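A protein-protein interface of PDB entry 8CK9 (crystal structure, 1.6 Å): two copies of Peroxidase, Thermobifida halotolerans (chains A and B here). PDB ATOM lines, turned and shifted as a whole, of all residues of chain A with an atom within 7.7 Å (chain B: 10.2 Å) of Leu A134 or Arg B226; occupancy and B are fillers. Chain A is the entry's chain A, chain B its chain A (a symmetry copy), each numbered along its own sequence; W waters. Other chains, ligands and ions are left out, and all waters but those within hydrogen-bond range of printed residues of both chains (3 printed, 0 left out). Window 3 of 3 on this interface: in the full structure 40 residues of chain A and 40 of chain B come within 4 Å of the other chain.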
ATOM      1  N   LEU A  58      25.144  -5.167 -26.279  1.00  0.00           N
ATOM      2  CA  LEU A  58      24.619  -3.807 -26.298  1.00  0.00           C
ATOM      3  C   LEU A  58      25.622  -2.761 -26.774  1.00  0.00           C
ATOM      4  O   LEU A  58      25.204  -1.645 -27.114  1.00  0.00           O
ATOM      5  CB  LEU A  58      24.115  -3.416 -24.900  1.00  0.00           C
ATOM      6  CG  LEU A  58      22.799  -4.061 -24.455  1.00  0.00           C
ATOM      7  CD1 LEU A  58      22.467  -3.667 -23.024  1.00  0.00           C
ATOM      8  CD2 LEU A  58      21.671  -3.674 -25.398  1.00  0.00           C
ATOM      9  N   ARG A  59      26.917  -3.088 -26.826  1.00  0.00           N
ATOM     10  CA  ARG A  59      27.944  -2.069 -27.046  1.00  0.00           C
ATOM     11  C   ARG A  59      27.783  -1.383 -28.400  1.00  0.00           C
ATOM     12  O   ARG A  59      27.844  -0.151 -28.494  1.00  0.00           O
ATOM     13  CB  ARG A  59      29.340  -2.689 -26.921  1.00  0.00           C
ATOM     14  CG  ARG A  59      30.479  -1.755 -27.334  1.00  0.00           C
ATOM     15  CD  ARG A  59      31.856  -2.409 -27.194  1.00  0.00           C
ATOM     16  NE  ARG A  59      32.126  -3.407 -28.226  1.00  0.00           N
ATOM     17  CZ  ARG A  59      32.772  -3.168 -29.360  1.00  0.00           C
ATOM     18  NH1 ARG A  59      33.209  -1.955 -29.666  1.00  0.00           N
ATOM     19  NH2 ARG A  59      32.993  -4.170 -30.207  1.00  0.00           N
ATOM     20  N   MET A  60      27.587  -2.163 -29.466  1.00  0.00           N
ATOM     21  CA  MET A  60      27.555  -1.577 -30.802  1.00  0.00           C
ATOM     22  C   MET A  60      26.388  -0.615 -30.960  1.00  0.00           C
ATOM     23  O   MET A  60      26.517   0.430 -31.609  1.00  0.00           O
ATOM     24  CB  MET A  60      27.486  -2.674 -31.866  1.00  0.00           C
ATOM     25  CG  MET A  60      28.755  -3.505 -31.984  1.00  0.00           C
ATOM     26  SD  MET A  60      30.201  -2.482 -32.338  1.00  0.00           S
ATOM     27  CE  MET A  60      29.853  -1.975 -34.028  1.00  0.00           C
ATOM     28  N   ALA A  61      25.239  -0.943 -30.372  1.00  0.00           N
ATOM     29  CA  ALA A  61      24.072  -0.087 -30.510  1.00  0.00           C
ATOM     30  C   ALA A  61      24.127   1.114 -29.572  1.00  0.00           C
ATOM     31  O   ALA A  61      23.499   2.138 -29.863  1.00  0.00           O
ATOM     32  CB  ALA A  61      22.797  -0.899 -30.256  1.00  0.00           C
ATOM     33  N   GLY A  62      24.883   1.023 -28.482  1.00  0.00           N
ATOM     34  CA  GLY A  62      24.844   2.055 -27.463  1.00  0.00           C
ATOM     35  C   GLY A  62      26.003   3.033 -27.460  1.00  0.00           C
ATOM     36  O   GLY A  62      25.961   4.022 -26.720  1.00  0.00           O
ATOM     37  N   GLN A  63      27.041   2.783 -28.274  1.00  0.00           N
ATOM     38  CA  GLN A  63      28.251   3.596 -28.242  1.00  0.00           C
ATOM     39  C   GLN A  63      28.477   4.315 -29.566  1.00  0.00           C
ATOM     40  O   GLN A  63      28.071   3.827 -30.618  1.00  0.00           O
ATOM     41  CB  GLN A  63      29.484   2.734 -27.928  1.00  0.00           C
ATOM     42  CG  GLN A  63      29.487   2.129 -26.527  1.00  0.00           C
ATOM     43  CD  GLN A  63      29.393   3.183 -25.437  1.00  0.00           C
ATOM     44  OE1 GLN A  63      28.642   3.031 -24.471  1.00  0.00           O
ATOM     45  NE2 GLN A  63      30.160   4.258 -25.584  1.00  0.00           N
ATOM     46  N   PRO A  64      29.137   5.470 -29.551  1.00  0.00           N
ATOM     47  CA  PRO A  64      29.551   6.089 -30.813  1.00  0.00           C
ATOM     48  C   PRO A  64      30.723   5.338 -31.421  1.00  0.00           C
ATOM     49  O   PRO A  64      31.478   4.641 -30.738  1.00  0.00           O
ATOM     50  CB  PRO A  64      29.957   7.515 -30.410  1.00  0.00           C
ATOM     51  CG  PRO A  64      29.789   7.608 -28.919  1.00  0.00           C
ATOM     52  CD  PRO A  64      29.604   6.227 -28.377  1.00  0.00           C
ATOM     53  N   ASP A 122      27.533  14.025 -32.489  1.00  0.00           N
ATOM     54  CA  ASP A 122      26.211  14.186 -31.886  1.00  0.00           C
ATOM     55  C   ASP A 122      25.123  13.281 -32.456  1.00  0.00           C
ATOM     56  O   ASP A 122      24.037  13.208 -31.863  1.00  0.00           O
ATOM     57  CB  ASP A 122      25.739  15.641 -32.034  1.00  0.00           C
ATOM     58  CG  ASP A 122      26.659  16.626 -31.352  1.00  0.00           C
ATOM     59  OD1 ASP A 122      26.980  16.414 -30.165  1.00  0.00           O
ATOM     60  OD2 ASP A 122      27.066  17.608 -32.010  1.00  0.00           O
ATOM     61  N   GLY A 123      25.354  12.616 -33.586  1.00  0.00           N
ATOM     62  CA  GLY A 123      24.328  11.818 -34.221  1.00  0.00           C
ATOM     63  C   GLY A 123      23.438  12.638 -35.135  1.00  0.00           C
ATOM     64  O   GLY A 123      23.596  13.859 -35.255  1.00  0.00           O
ATOM     65  N   PRO A 124      22.498  11.980 -35.823  1.00  0.00           N
ATOM     66  CA  PRO A 124      21.524  12.727 -36.630  1.00  0.00           C
ATOM     67  C   PRO A 124      20.724  13.676 -35.757  1.00  0.00           C
ATOM     68  O   PRO A 124      20.470  13.410 -34.582  1.00  0.00           O
ATOM     69  CB  PRO A 124      20.635  11.632 -37.239  1.00  0.00           C
ATOM     70  CG  PRO A 124      21.520  10.387 -37.235  1.00  0.00           C
ATOM     71  CD  PRO A 124      22.340  10.521 -35.966  1.00  0.00           C
ATOM     72  N   ALA A 130      15.935   9.428 -36.409  1.00  0.00           N
ATOM     73  CA  ALA A 130      16.774   8.836 -35.377  1.00  0.00           C
ATOM     74  C   ALA A 130      16.665   9.547 -34.034  1.00  0.00           C
ATOM     75  O   ALA A 130      17.393   9.199 -33.098  1.00  0.00           O
ATOM     76  CB  ALA A 130      18.234   8.804 -35.831  1.00  0.00           C
ATOM     77  N   THR A 131      15.776  10.532 -33.911  1.00  0.00           N
ATOM     78  CA  THR A 131      15.590  11.181 -32.618  1.00  0.00           C
ATOM     79  C   THR A 131      15.171  10.163 -31.565  1.00  0.00           C
ATOM     80  O   THR A 131      14.300   9.322 -31.807  1.00  0.00           O
ATOM     81  CB  THR A 131      14.543  12.283 -32.739  1.00  0.00           C
ATOM     82  OG1 THR A 131      14.946  13.208 -33.757  1.00  0.00           O
ATOM     83  CG2 THR A 131      14.393  13.013 -31.418  1.00  0.00           C
ATOM     84  N   GLY A 132      15.806  10.231 -30.395  1.00  0.00           N
ATOM     85  CA  GLY A 132      15.528   9.303 -29.322  1.00  0.00           C
ATOM     86  C   GLY A 132      16.341   8.030 -29.346  1.00  0.00           C
ATOM     87  O   GLY A 132      16.121   7.156 -28.495  1.00  0.00           O
ATOM     88  N   LEU A 133      17.270   7.892 -30.287  1.00  0.00           N
ATOM     89  CA  LEU A 133      18.080   6.691 -30.396  1.00  0.00           C
ATOM     90  C   LEU A 133      19.514   6.963 -29.963  1.00  0.00           C
ATOM     91  O   LEU A 133      20.008   8.091 -30.030  1.00  0.00           O
ATOM     92  CB  LEU A 133      18.068   6.155 -31.831  1.00  0.00           C
ATOM     93  CG  LEU A 133      16.671   5.868 -32.388  1.00  0.00           C
ATOM     94  CD1 LEU A 133      16.776   5.329 -33.814  1.00  0.00           C
ATOM     95  CD2 LEU A 133      15.901   4.894 -31.497  1.00  0.00           C
ATOM     96  N   LEU A 134      20.177   5.890 -29.534  1.00  0.00           N
ATOM     97  CA  LEU A 134      21.573   5.921 -29.133  1.00  0.00           C
ATOM     98  C   LEU A 134      22.459   6.080 -30.375  1.00  0.00           C
ATOM     99  O   LEU A 134      21.983   5.977 -31.509  1.00  0.00           O
ATOM    100  CB  LEU A 134      21.899   4.641 -28.358  1.00  0.00           C
ATOM    101  CG  LEU A 134      21.184   4.549 -27.009  1.00  0.00           C
ATOM    102  CD1 LEU A 134      21.165   3.121 -26.525  1.00  0.00           C
ATOM    103  CD2 LEU A 134      21.904   5.450 -26.013  1.00  0.00           C
ATOM    104  N   PRO A 135      23.756   6.344 -30.197  1.00  0.00           N
ATOM    105  CA  PRO A 135      24.595   6.652 -31.369  1.00  0.00           C
ATOM    106  C   PRO A 135      24.766   5.493 -32.332  1.00  0.00           C
ATOM    107  O   PRO A 135      24.990   5.723 -33.531  1.00  0.00           O
ATOM    108  CB  PRO A 135      25.937   7.059 -30.743  1.00  0.00           C
ATOM    109  CG  PRO A 135      25.581   7.502 -29.356  1.00  0.00           C
ATOM    110  CD  PRO A 135      24.472   6.593 -28.932  1.00  0.00           C
ATOM    111  N   ALA A 136      24.687   4.256 -31.838  1.00  0.00           N
ATOM    112  CA  ALA A 136      24.675   3.062 -32.687  1.00  0.00           C
ATOM    113  C   ALA A 136      25.875   3.004 -33.632  1.00  0.00           C
ATOM    114  O   ALA A 136      25.764   2.580 -34.784  1.00  0.00           O
ATOM    115  CB  ALA A 136      23.361   2.971 -33.468  1.00  0.00           C
ATOM    116  N   SER A 137      27.039   3.426 -33.134  1.00  0.00           N
ATOM    117  CA  SER A 137      28.306   3.266 -33.848  1.00  0.00           C
ATOM    118  C   SER A 137      28.273   3.896 -35.242  1.00  0.00           C
ATOM    119  O   SER A 137      28.892   3.381 -36.170  1.00  0.00           O
ATOM    120  CB  SER A 137      28.694   1.786 -33.947  1.00  0.00           C
ATOM    121  OG  SER A 137      28.792   1.204 -32.652  1.00  0.00           O
ATOM    122  N   LEU A 138      27.551   5.009 -35.402  1.00  0.00           N
ATOM    123  CA  LEU A 138      27.442   5.646 -36.712  1.00  0.00           C
ATOM    124  C   LEU A 138      28.813   6.070 -37.223  1.00  0.00           C
ATOM    125  O   LEU A 138      29.574   6.735 -36.512  1.00  0.00           O
ATOM    126  CB  LEU A 138      26.513   6.856 -36.628  1.00  0.00           C
ATOM    127  CG  LEU A 138      26.302   7.670 -37.903  1.00  0.00           C
ATOM    128  CD1 LEU A 138      25.696   6.833 -39.035  1.00  0.00           C
ATOM    129  CD2 LEU A 138      25.410   8.873 -37.595  1.00  0.00           C
ATOM    130  N   ALA A 188      26.043   1.810 -39.388  1.00  0.00           N
ATOM    131  CA  ALA A 188      25.479   1.969 -38.052  1.00  0.00           C
ATOM    132  C   ALA A 188      24.917   0.635 -37.592  1.00  0.00           C
ATOM    133  O   ALA A 188      24.672  -0.271 -38.397  1.00  0.00           O
ATOM    134  CB  ALA A 188      24.387   3.047 -38.024  1.00  0.00           C
ATOM    135  N   ASP A 190      22.040   0.404 -36.137  1.00  0.00           N
ATOM    136  CA  ASP A 190      20.604   0.560 -36.173  1.00  0.00           C
ATOM    137  C   ASP A 190      20.158   1.119 -37.518  1.00  0.00           C
ATOM    138  O   ASP A 190      20.762   2.075 -38.027  1.00  0.00           O
ATOM    139  CB  ASP A 190      20.152   1.496 -35.056  1.00  0.00           C
ATOM    140  CG  ASP A 190      18.666   1.626 -35.011  1.00  0.00           C
ATOM    141  OD1 ASP A 190      18.033   0.813 -34.305  1.00  0.00           O
ATOM    142  OD2 ASP A 190      18.140   2.510 -35.713  1.00  0.00           O
ATOM    143  N   VAL A 193      18.993   4.946 -37.389  1.00  0.00           N
ATOM    144  CA  VAL A 193      20.146   5.838 -37.319  1.00  0.00           C
ATOM    145  C   VAL A 193      20.796   5.950 -38.691  1.00  0.00           C
ATOM    146  O   VAL A 193      21.113   7.052 -39.166  1.00  0.00           O
ATOM    147  CB  VAL A 193      21.135   5.335 -36.254  1.00  0.00           C
ATOM    148  CG1 VAL A 193      22.433   6.142 -36.309  1.00  0.00           C
ATOM    149  CG2 VAL A 193      20.499   5.438 -34.877  1.00  0.00           C
ATOM    150  N   ALA B  54      18.567  -1.951 -19.824  1.00  0.00           N
ATOM    151  CA  ALA B  54      19.345  -2.970 -20.523  1.00  0.00           C
ATOM    152  C   ALA B  54      18.510  -4.214 -20.833  1.00  0.00           C
ATOM    153  O   ALA B  54      18.596  -4.771 -21.932  1.00  0.00           O
ATOM    154  CB  ALA B  54      20.572  -3.351 -19.709  1.00  0.00           C
ATOM    155  N   GLU B  55      17.701  -4.651 -19.862  1.00  0.00           N
ATOM    156  CA  GLU B  55      16.875  -5.840 -20.069  1.00  0.00           C
ATOM    157  C   GLU B  55      15.903  -5.644 -21.226  1.00  0.00           C
ATOM    158  O   GLU B  55      15.754  -6.525 -22.081  1.00  0.00           O
ATOM    159  CB  GLU B  55      16.120  -6.193 -18.784  1.00  0.00           C
ATOM    160  CG  GLU B  55      14.909  -7.092 -19.005  1.00  0.00           C
ATOM    161  CD  GLU B  55      14.299  -7.588 -17.707  1.00  0.00           C
ATOM    162  OE1 GLU B  55      15.050  -8.116 -16.859  1.00  0.00           O
ATOM    163  OE2 GLU B  55      13.070  -7.448 -17.532  1.00  0.00           O
ATOM    164  N   GLU B  56      15.231  -4.490 -21.275  1.00  0.00           N
ATOM    165  CA  GLU B  56      14.299  -4.234 -22.366  1.00  0.00           C
ATOM    166  C   GLU B  56      15.010  -3.953 -23.684  1.00  0.00           C
ATOM    167  O   GLU B  56      14.418  -4.166 -24.749  1.00  0.00           O
ATOM    168  CB  GLU B  56      13.362  -3.076 -22.011  1.00  0.00           C
ATOM    169  CG  GLU B  56      12.261  -3.448 -21.022  1.00  0.00           C
ATOM    170  CD  GLU B  56      11.066  -2.510 -21.096  1.00  0.00           C
ATOM    171  OE1 GLU B  56      11.129  -1.520 -21.859  1.00  0.00           O
ATOM    172  OE2 GLU B  56      10.060  -2.766 -20.398  1.00  0.00           O
ATOM    173  N   ARG B  57      16.256  -3.479 -23.641  1.00  0.00           N
ATOM    174  CA  ARG B  57      17.017  -3.323 -24.876  1.00  0.00           C
ATOM    175  C   ARG B  57      17.361  -4.672 -25.494  1.00  0.00           C
ATOM    176  O   ARG B  57      17.467  -4.783 -26.720  1.00  0.00           O
ATOM    177  CB  ARG B  57      18.300  -2.525 -24.620  1.00  0.00           C
ATOM    178  CG  ARG B  57      18.097  -1.027 -24.418  1.00  0.00           C
ATOM    179  CD  ARG B  57      19.426  -0.321 -24.121  1.00  0.00           C
ATOM    180  NE  ARG B  57      20.380  -0.425 -25.221  1.00  0.00           N
ATOM    181  CZ  ARG B  57      21.663  -0.098 -25.135  1.00  0.00           C
ATOM    182  NH1 ARG B  57      22.192   0.349 -24.004  1.00  0.00           N
ATOM    183  NH2 ARG B  57      22.441  -0.231 -26.207  1.00  0.00           N
ATOM    184  N   LEU B  58      17.526  -5.706 -24.669  1.00  0.00           N
ATOM    185  CA  LEU B  58      17.944  -7.020 -25.145  1.00  0.00           C
ATOM    186  C   LEU B  58      16.793  -8.003 -25.343  1.00  0.00           C
ATOM    187  O   LEU B  58      16.991  -9.023 -26.018  1.00  0.00           O
ATOM    188  CB  LEU B  58      18.963  -7.634 -24.174  1.00  0.00           C
ATOM    189  CG  LEU B  58      20.371  -7.028 -24.205  1.00  0.00           C
ATOM    190  CD1 LEU B  58      21.248  -7.657 -23.134  1.00  0.00           C
ATOM    191  CD2 LEU B  58      20.993  -7.197 -25.581  1.00  0.00           C
ATOM    192  N   ARG B  78       4.926  -7.011 -28.523  1.00  0.00           N
ATOM    193  CA  ARG B  78       5.792  -5.979 -29.071  1.00  0.00           C
ATOM    194  C   ARG B  78       6.131  -6.308 -30.520  1.00  0.00           C
ATOM    195  O   ARG B  78       6.422  -7.457 -30.864  1.00  0.00           O
ATOM    196  CB  ARG B  78       7.069  -5.846 -28.245  1.00  0.00           C
ATOM    197  CG  ARG B  78       7.983  -4.730 -28.743  1.00  0.00           C
ATOM    198  CD  ARG B  78       9.021  -4.348 -27.707  1.00  0.00           C
ATOM    199  NE  ARG B  78       9.971  -3.366 -28.215  1.00  0.00           N
ATOM    200  CZ  ARG B  78       9.752  -2.058 -28.239  1.00  0.00           C
ATOM    201  NH1 ARG B  78       8.603  -1.545 -27.828  1.00  0.00           N
ATOM    202  NH2 ARG B  78      10.710  -1.247 -28.679  1.00  0.00           N
ATOM    203  N   HIS B 220      13.215   1.212 -35.586  1.00  0.00           N
ATOM    204  CA  HIS B 220      14.431   1.176 -34.794  1.00  0.00           C
ATOM    205  C   HIS B 220      14.503  -0.136 -34.028  1.00  0.00           C
ATOM    206  O   HIS B 220      13.483  -0.787 -33.759  1.00  0.00           O
ATOM    207  CB  HIS B 220      14.489   2.353 -33.825  1.00  0.00           C
ATOM    208  CG  HIS B 220      13.512   2.246 -32.696  1.00  0.00           C
ATOM    209  ND1 HIS B 220      13.805   1.604 -31.514  1.00  0.00           N
ATOM    210  CD2 HIS B 220      12.239   2.692 -32.577  1.00  0.00           C
ATOM    211  CE1 HIS B 220      12.756   1.661 -30.711  1.00  0.00           C
ATOM    212  NE2 HIS B 220      11.794   2.322 -31.331  1.00  0.00           N
ATOM    213  N   THR B 221      15.724  -0.537 -33.691  1.00  0.00           N
ATOM    214  CA  THR B 221      15.929  -1.734 -32.892  1.00  0.00           C
ATOM    215  C   THR B 221      15.807  -1.398 -31.413  1.00  0.00           C
ATOM    216  O   THR B 221      16.153  -0.301 -30.969  1.00  0.00           O
ATOM    217  CB  THR B 221      17.301  -2.368 -33.152  1.00  0.00           C
ATOM    218  OG1 THR B 221      18.334  -1.444 -32.780  1.00  0.00           O
ATOM    219  CG2 THR B 221      17.462  -2.773 -34.619  1.00  0.00           C
ATOM    220  N   ALA B 222      15.297  -2.361 -30.646  1.00  0.00           N
ATOM    221  CA  ALA B 222      15.172  -2.145 -29.211  1.00  0.00           C
ATOM    222  C   ALA B 222      16.521  -1.814 -28.592  1.00  0.00           C
ATOM    223  O   ALA B 222      16.608  -0.985 -27.680  1.00  0.00           O
ATOM    224  CB  ALA B 222      14.568  -3.380 -28.546  1.00  0.00           C
ATOM    225  N   ALA B 223      17.591  -2.436 -29.092  1.00  0.00           N
ATOM    226  CA  ALA B 223      18.910  -2.220 -28.505  1.00  0.00           C
ATOM    227  C   ALA B 223      19.360  -0.766 -28.613  1.00  0.00           C
ATOM    228  O   ALA B 223      20.160  -0.309 -27.795  1.00  0.00           O
ATOM    229  CB  ALA B 223      19.928  -3.138 -29.175  1.00  0.00           C
ATOM    230  N   ALA B 224      18.850  -0.021 -29.590  1.00  0.00           N
ATOM    231  CA  ALA B 224      19.279   1.356 -29.814  1.00  0.00           C
ATOM    232  C   ALA B 224      18.345   2.392 -29.197  1.00  0.00           C
ATOM    233  O   ALA B 224      18.590   3.595 -29.349  1.00  0.00           O
ATOM    234  CB  ALA B 224      19.424   1.630 -31.319  1.00  0.00           C
ATOM    235  N   ALA B 225      17.292   1.972 -28.503  1.00  0.00           N
ATOM    236  CA  ALA B 225      16.340   2.917 -27.939  1.00  0.00           C
ATOM    237  C   ALA B 225      16.876   3.471 -26.625  1.00  0.00           C
ATOM    238  O   ALA B 225      17.190   2.704 -25.708  1.00  0.00           O
ATOM    239  CB  ALA B 225      14.989   2.243 -27.719  1.00  0.00           C
ATOM    240  N   ARG B 226      16.978   4.797 -26.532  1.00  0.00           N
ATOM    241  CA  ARG B 226      17.283   5.413 -25.242  1.00  0.00           C
ATOM    242  C   ARG B 226      16.217   5.060 -24.213  1.00  0.00           C
ATOM    243  O   ARG B 226      16.532   4.754 -23.057  1.00  0.00           O
ATOM    244  CB  ARG B 226      17.411   6.928 -25.396  1.00  0.00           C
ATOM    245  CG  ARG B 226      18.594   7.361 -26.245  1.00  0.00           C
ATOM    246  CD  ARG B 226      18.764   8.875 -26.297  1.00  0.00           C
ATOM    247  NE  ARG B 226      20.010   9.230 -26.966  1.00  0.00           N
ATOM    248  CZ  ARG B 226      21.205   9.200 -26.390  1.00  0.00           C
ATOM    249  NH1 ARG B 226      21.349   8.885 -25.113  1.00  0.00           N
ATOM    250  NH2 ARG B 226      22.285   9.487 -27.117  1.00  0.00           N
ATOM    251  N   ASN B 227      14.952   5.077 -24.625  1.00  0.00           N
ATOM    252  CA  ASN B 227      13.826   4.675 -23.782  1.00  0.00           C
ATOM    253  C   ASN B 227      13.082   3.565 -24.507  1.00  0.00           C
ATOM    254  O   ASN B 227      12.319   3.837 -25.451  1.00  0.00           O
ATOM    255  CB  ASN B 227      12.908   5.863 -23.500  1.00  0.00           C
ATOM    256  CG  ASN B 227      11.628   5.465 -22.780  1.00  0.00           C
ATOM    257  OD1 ASN B 227      11.478   4.333 -22.316  1.00  0.00           O
ATOM    258  ND2 ASN B 227      10.692   6.406 -22.689  1.00  0.00           N
ATOM    259  N   PRO B 228      13.262   2.305 -24.108  1.00  0.00           N
ATOM    260  CA  PRO B 228      12.709   1.196 -24.904  1.00  0.00           C
ATOM    261  C   PRO B 228      11.190   1.182 -24.977  1.00  0.00           C
ATOM    262  O   PRO B 228      10.639   0.572 -25.901  1.00  0.00           O
ATOM    263  CB  PRO B 228      13.254  -0.049 -24.191  1.00  0.00           C
ATOM    264  CG  PRO B 228      13.548   0.410 -22.798  1.00  0.00           C
ATOM    265  CD  PRO B 228      13.996   1.833 -22.922  1.00  0.00           C
ATOM    266  N   ASP B 229      10.500   1.848 -24.057  1.00  0.00           N
ATOM    267  CA  ASP B 229       9.045   1.927 -24.097  1.00  0.00           C
ATOM    268  C   ASP B 229       8.529   3.084 -24.941  1.00  0.00           C
ATOM    269  O   ASP B 229       7.311   3.213 -25.100  1.00  0.00           O
ATOM    270  CB  ASP B 229       8.477   2.046 -22.679  1.00  0.00           C
ATOM    271  CG  ASP B 229       8.512   0.730 -21.926  1.00  0.00           C
ATOM    272  OD1 ASP B 229       8.584  -0.331 -22.581  1.00  0.00           O
ATOM    273  OD2 ASP B 229       8.459   0.761 -20.679  1.00  0.00           O
ATOM    274  N   ALA B 230       9.407   3.920 -25.482  1.00  0.00           N
ATOM    275  CA  ALA B 230       8.953   5.078 -26.239  1.00  0.00           C
ATOM    276  C   ALA B 230       8.339   4.652 -27.566  1.00  0.00           C
ATOM    277  O   ALA B 230       8.698   3.625 -28.149  1.00  0.00           O
ATOM    278  CB  ALA B 230      10.106   6.051 -26.480  1.00  0.00           C
ATOM    279  N   THR B 231       7.394   5.457 -28.033  1.00  0.00           N
ATOM    280  CA  THR B 231       6.747   5.213 -29.312  1.00  0.00           C
ATOM    281  C   THR B 231       7.757   5.401 -30.447  1.00  0.00           C
ATOM    282  O   THR B 231       8.567   6.331 -30.405  1.00  0.00           O
ATOM    283  CB  THR B 231       5.562   6.178 -29.459  1.00  0.00           C
ATOM    284  OG1 THR B 231       4.729   6.084 -28.291  1.00  0.00           O
ATOM    285  CG2 THR B 231       4.714   5.864 -30.690  1.00  0.00           C
ATOM    286  N   ARG B 233       9.400   6.296 -34.230  1.00  0.00           N
ATOM    287  CA  ARG B 233       9.258   7.367 -35.212  1.00  0.00           C
ATOM    288  C   ARG B 233       9.319   6.808 -36.630  1.00  0.00           C
ATOM    289  O   ARG B 233       9.835   5.713 -36.868  1.00  0.00           O
ATOM    290  CB  ARG B 233      10.342   8.439 -35.024  1.00  0.00           C
ATOM    291  CG  ARG B 233      10.215   9.202 -33.707  1.00  0.00           C
ATOM    292  CD  ARG B 233      11.309  10.250 -33.540  1.00  0.00           C
ATOM    293  NE  ARG B 233      11.215  10.956 -32.265  1.00  0.00           N
ATOM    294  CZ  ARG B 233      10.598  12.119 -32.095  1.00  0.00           C
ATOM    295  NH1 ARG B 233      10.001  12.739 -33.100  1.00  0.00           N
ATOM    296  NH2 ARG B 233      10.568  12.666 -30.882  1.00  0.00           N
HETATM  297  O   HOH W   1      18.711  10.828 -29.608  1.00  0.00           O
HETATM  298  O   HOH W   2      11.680   8.993 -29.724  1.00  0.00           O
HETATM  299  O   HOH W   3      14.103   6.383 -27.085  1.00  0.00           O
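The backbone NH of Leu A134 sits at hydrogen-bond distance from the backbone carbonyl oxygen of Ala B224, 2.8 Å away.
The backbone carbonyl oxygen (O) of Leu A58 sits at hydrogen-bond distance from the guanidinium group (NH2) of Arg B57.
The side-chain carboxylate (OD1) of Asp A190 sits at hydrogen-bond distance from the side-chain hydroxyl (OG1) of Thr B221 (2.7 Å).
NE of Arg B226 lies within hydrogen-bond range of O of Leu A133 (3.3 Å).
The backbone carbonyl oxygen (O) of Gly A132 lies within hydrogen-bond range of the backbone NH (N) of Arg B226, 3.2 Å away.
N of Ala A136 lies within hydrogen-bond range of O of Ala A61.
The side-chain carboxylate of Asp A190 lies within hydrogen-bond range of the backbone NH of Val A193 (3.1 Å).
The guanidinium group (NE) of Arg B57 sits at hydrogen-bond distance from the backbone carbonyl oxygen (O) of Ala B223, at 2.6 Å.
Among the printed residues, pairs that only touch across the chains: Leu A58 with Ala B54 (3.8 Å), Leu A58 with Leu B58 (3.6 Å), Ala A61 with Arg B57 (3.997 Å), Ala A61 with Ala B223 (3.7 Å), Gly A62 with Arg B57 (3.5 Å), Thr A131 with Arg B233 (3.5 Å), Leu A133 with His B220 (3.7 Å), Leu A133 with Ala B224 (3.3 Å), Leu A134 with Arg B57 (3.5 Å), Leu A134 with Ala B223 (3.8 Å), Leu A134 with Arg B226 (3.6 Å), Asp A190 with His B220 (3.7 Å) and Asp A190 with Ala B224 (3.4 Å).
Arg B226 touches just these residues of chain A: Gly A132 (3.2 Å), Leu A133 (3.3 Å) and Leu A134 (3.6 Å).
Of the printed residues of chain B, Leu A133 touches His B220 (3.7 Å), Ala B224 (3.3 Å) and Arg B226 (3.3 Å).
Printed residues of chain B within 4 Å of Asp A190: His B220 (3.7 Å), Thr B221 (2.7 Å) and Ala B224 (3.4 Å).
Printed residues of chain A within 4 Å of Arg B233: Thr A131.
Of the printed residues of chain B, Thr A131 touches Arg B233 (3.5 Å).
Pro A124 touches none of the printed residues of chain B.
The nearest residue of chain A that does not touch Arg B226 is Pro A135 (4.1 Å).
Along chain A the printed residues that touch a printed residue of chain B span positions 58 to 190.
Of the 19 printed residues of chain B, 9 touch a printed residue of chain A.
Printed residues of chain B that touch a printed residue of chain A: Ala B54, Arg B57, Leu B58, His B220, Thr B221, Ala B223, Ala B224, Arg B226 and Arg B233.
Hydrophobic or aromatic side chains of chain B that line the printed part of chain A: Ala B54, Leu B58, His B220, Ala B223 and Ala B224.
Leu B58 touches its own counterpart, Leu A58.
Position printed for both chains: 58.
Water W3 lies within hydrogen-bond range of the backbone carbonyl oxygen of Gly A132 (2.6 Å), the backbone NH of Asn B227 (2.9 Å) and the backbone NH of Arg B226 (3.3 Å).
Water W1 lies within hydrogen-bond range of O of Leu A133 (3.1 Å), N of Gly A132 (3.1 Å) and NE of Arg B226 (3.3 Å).
Water W2 lies within hydrogen-bond range of NE of Arg B233 (3.2 Å) and O of Thr A131 (3.4 Å).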
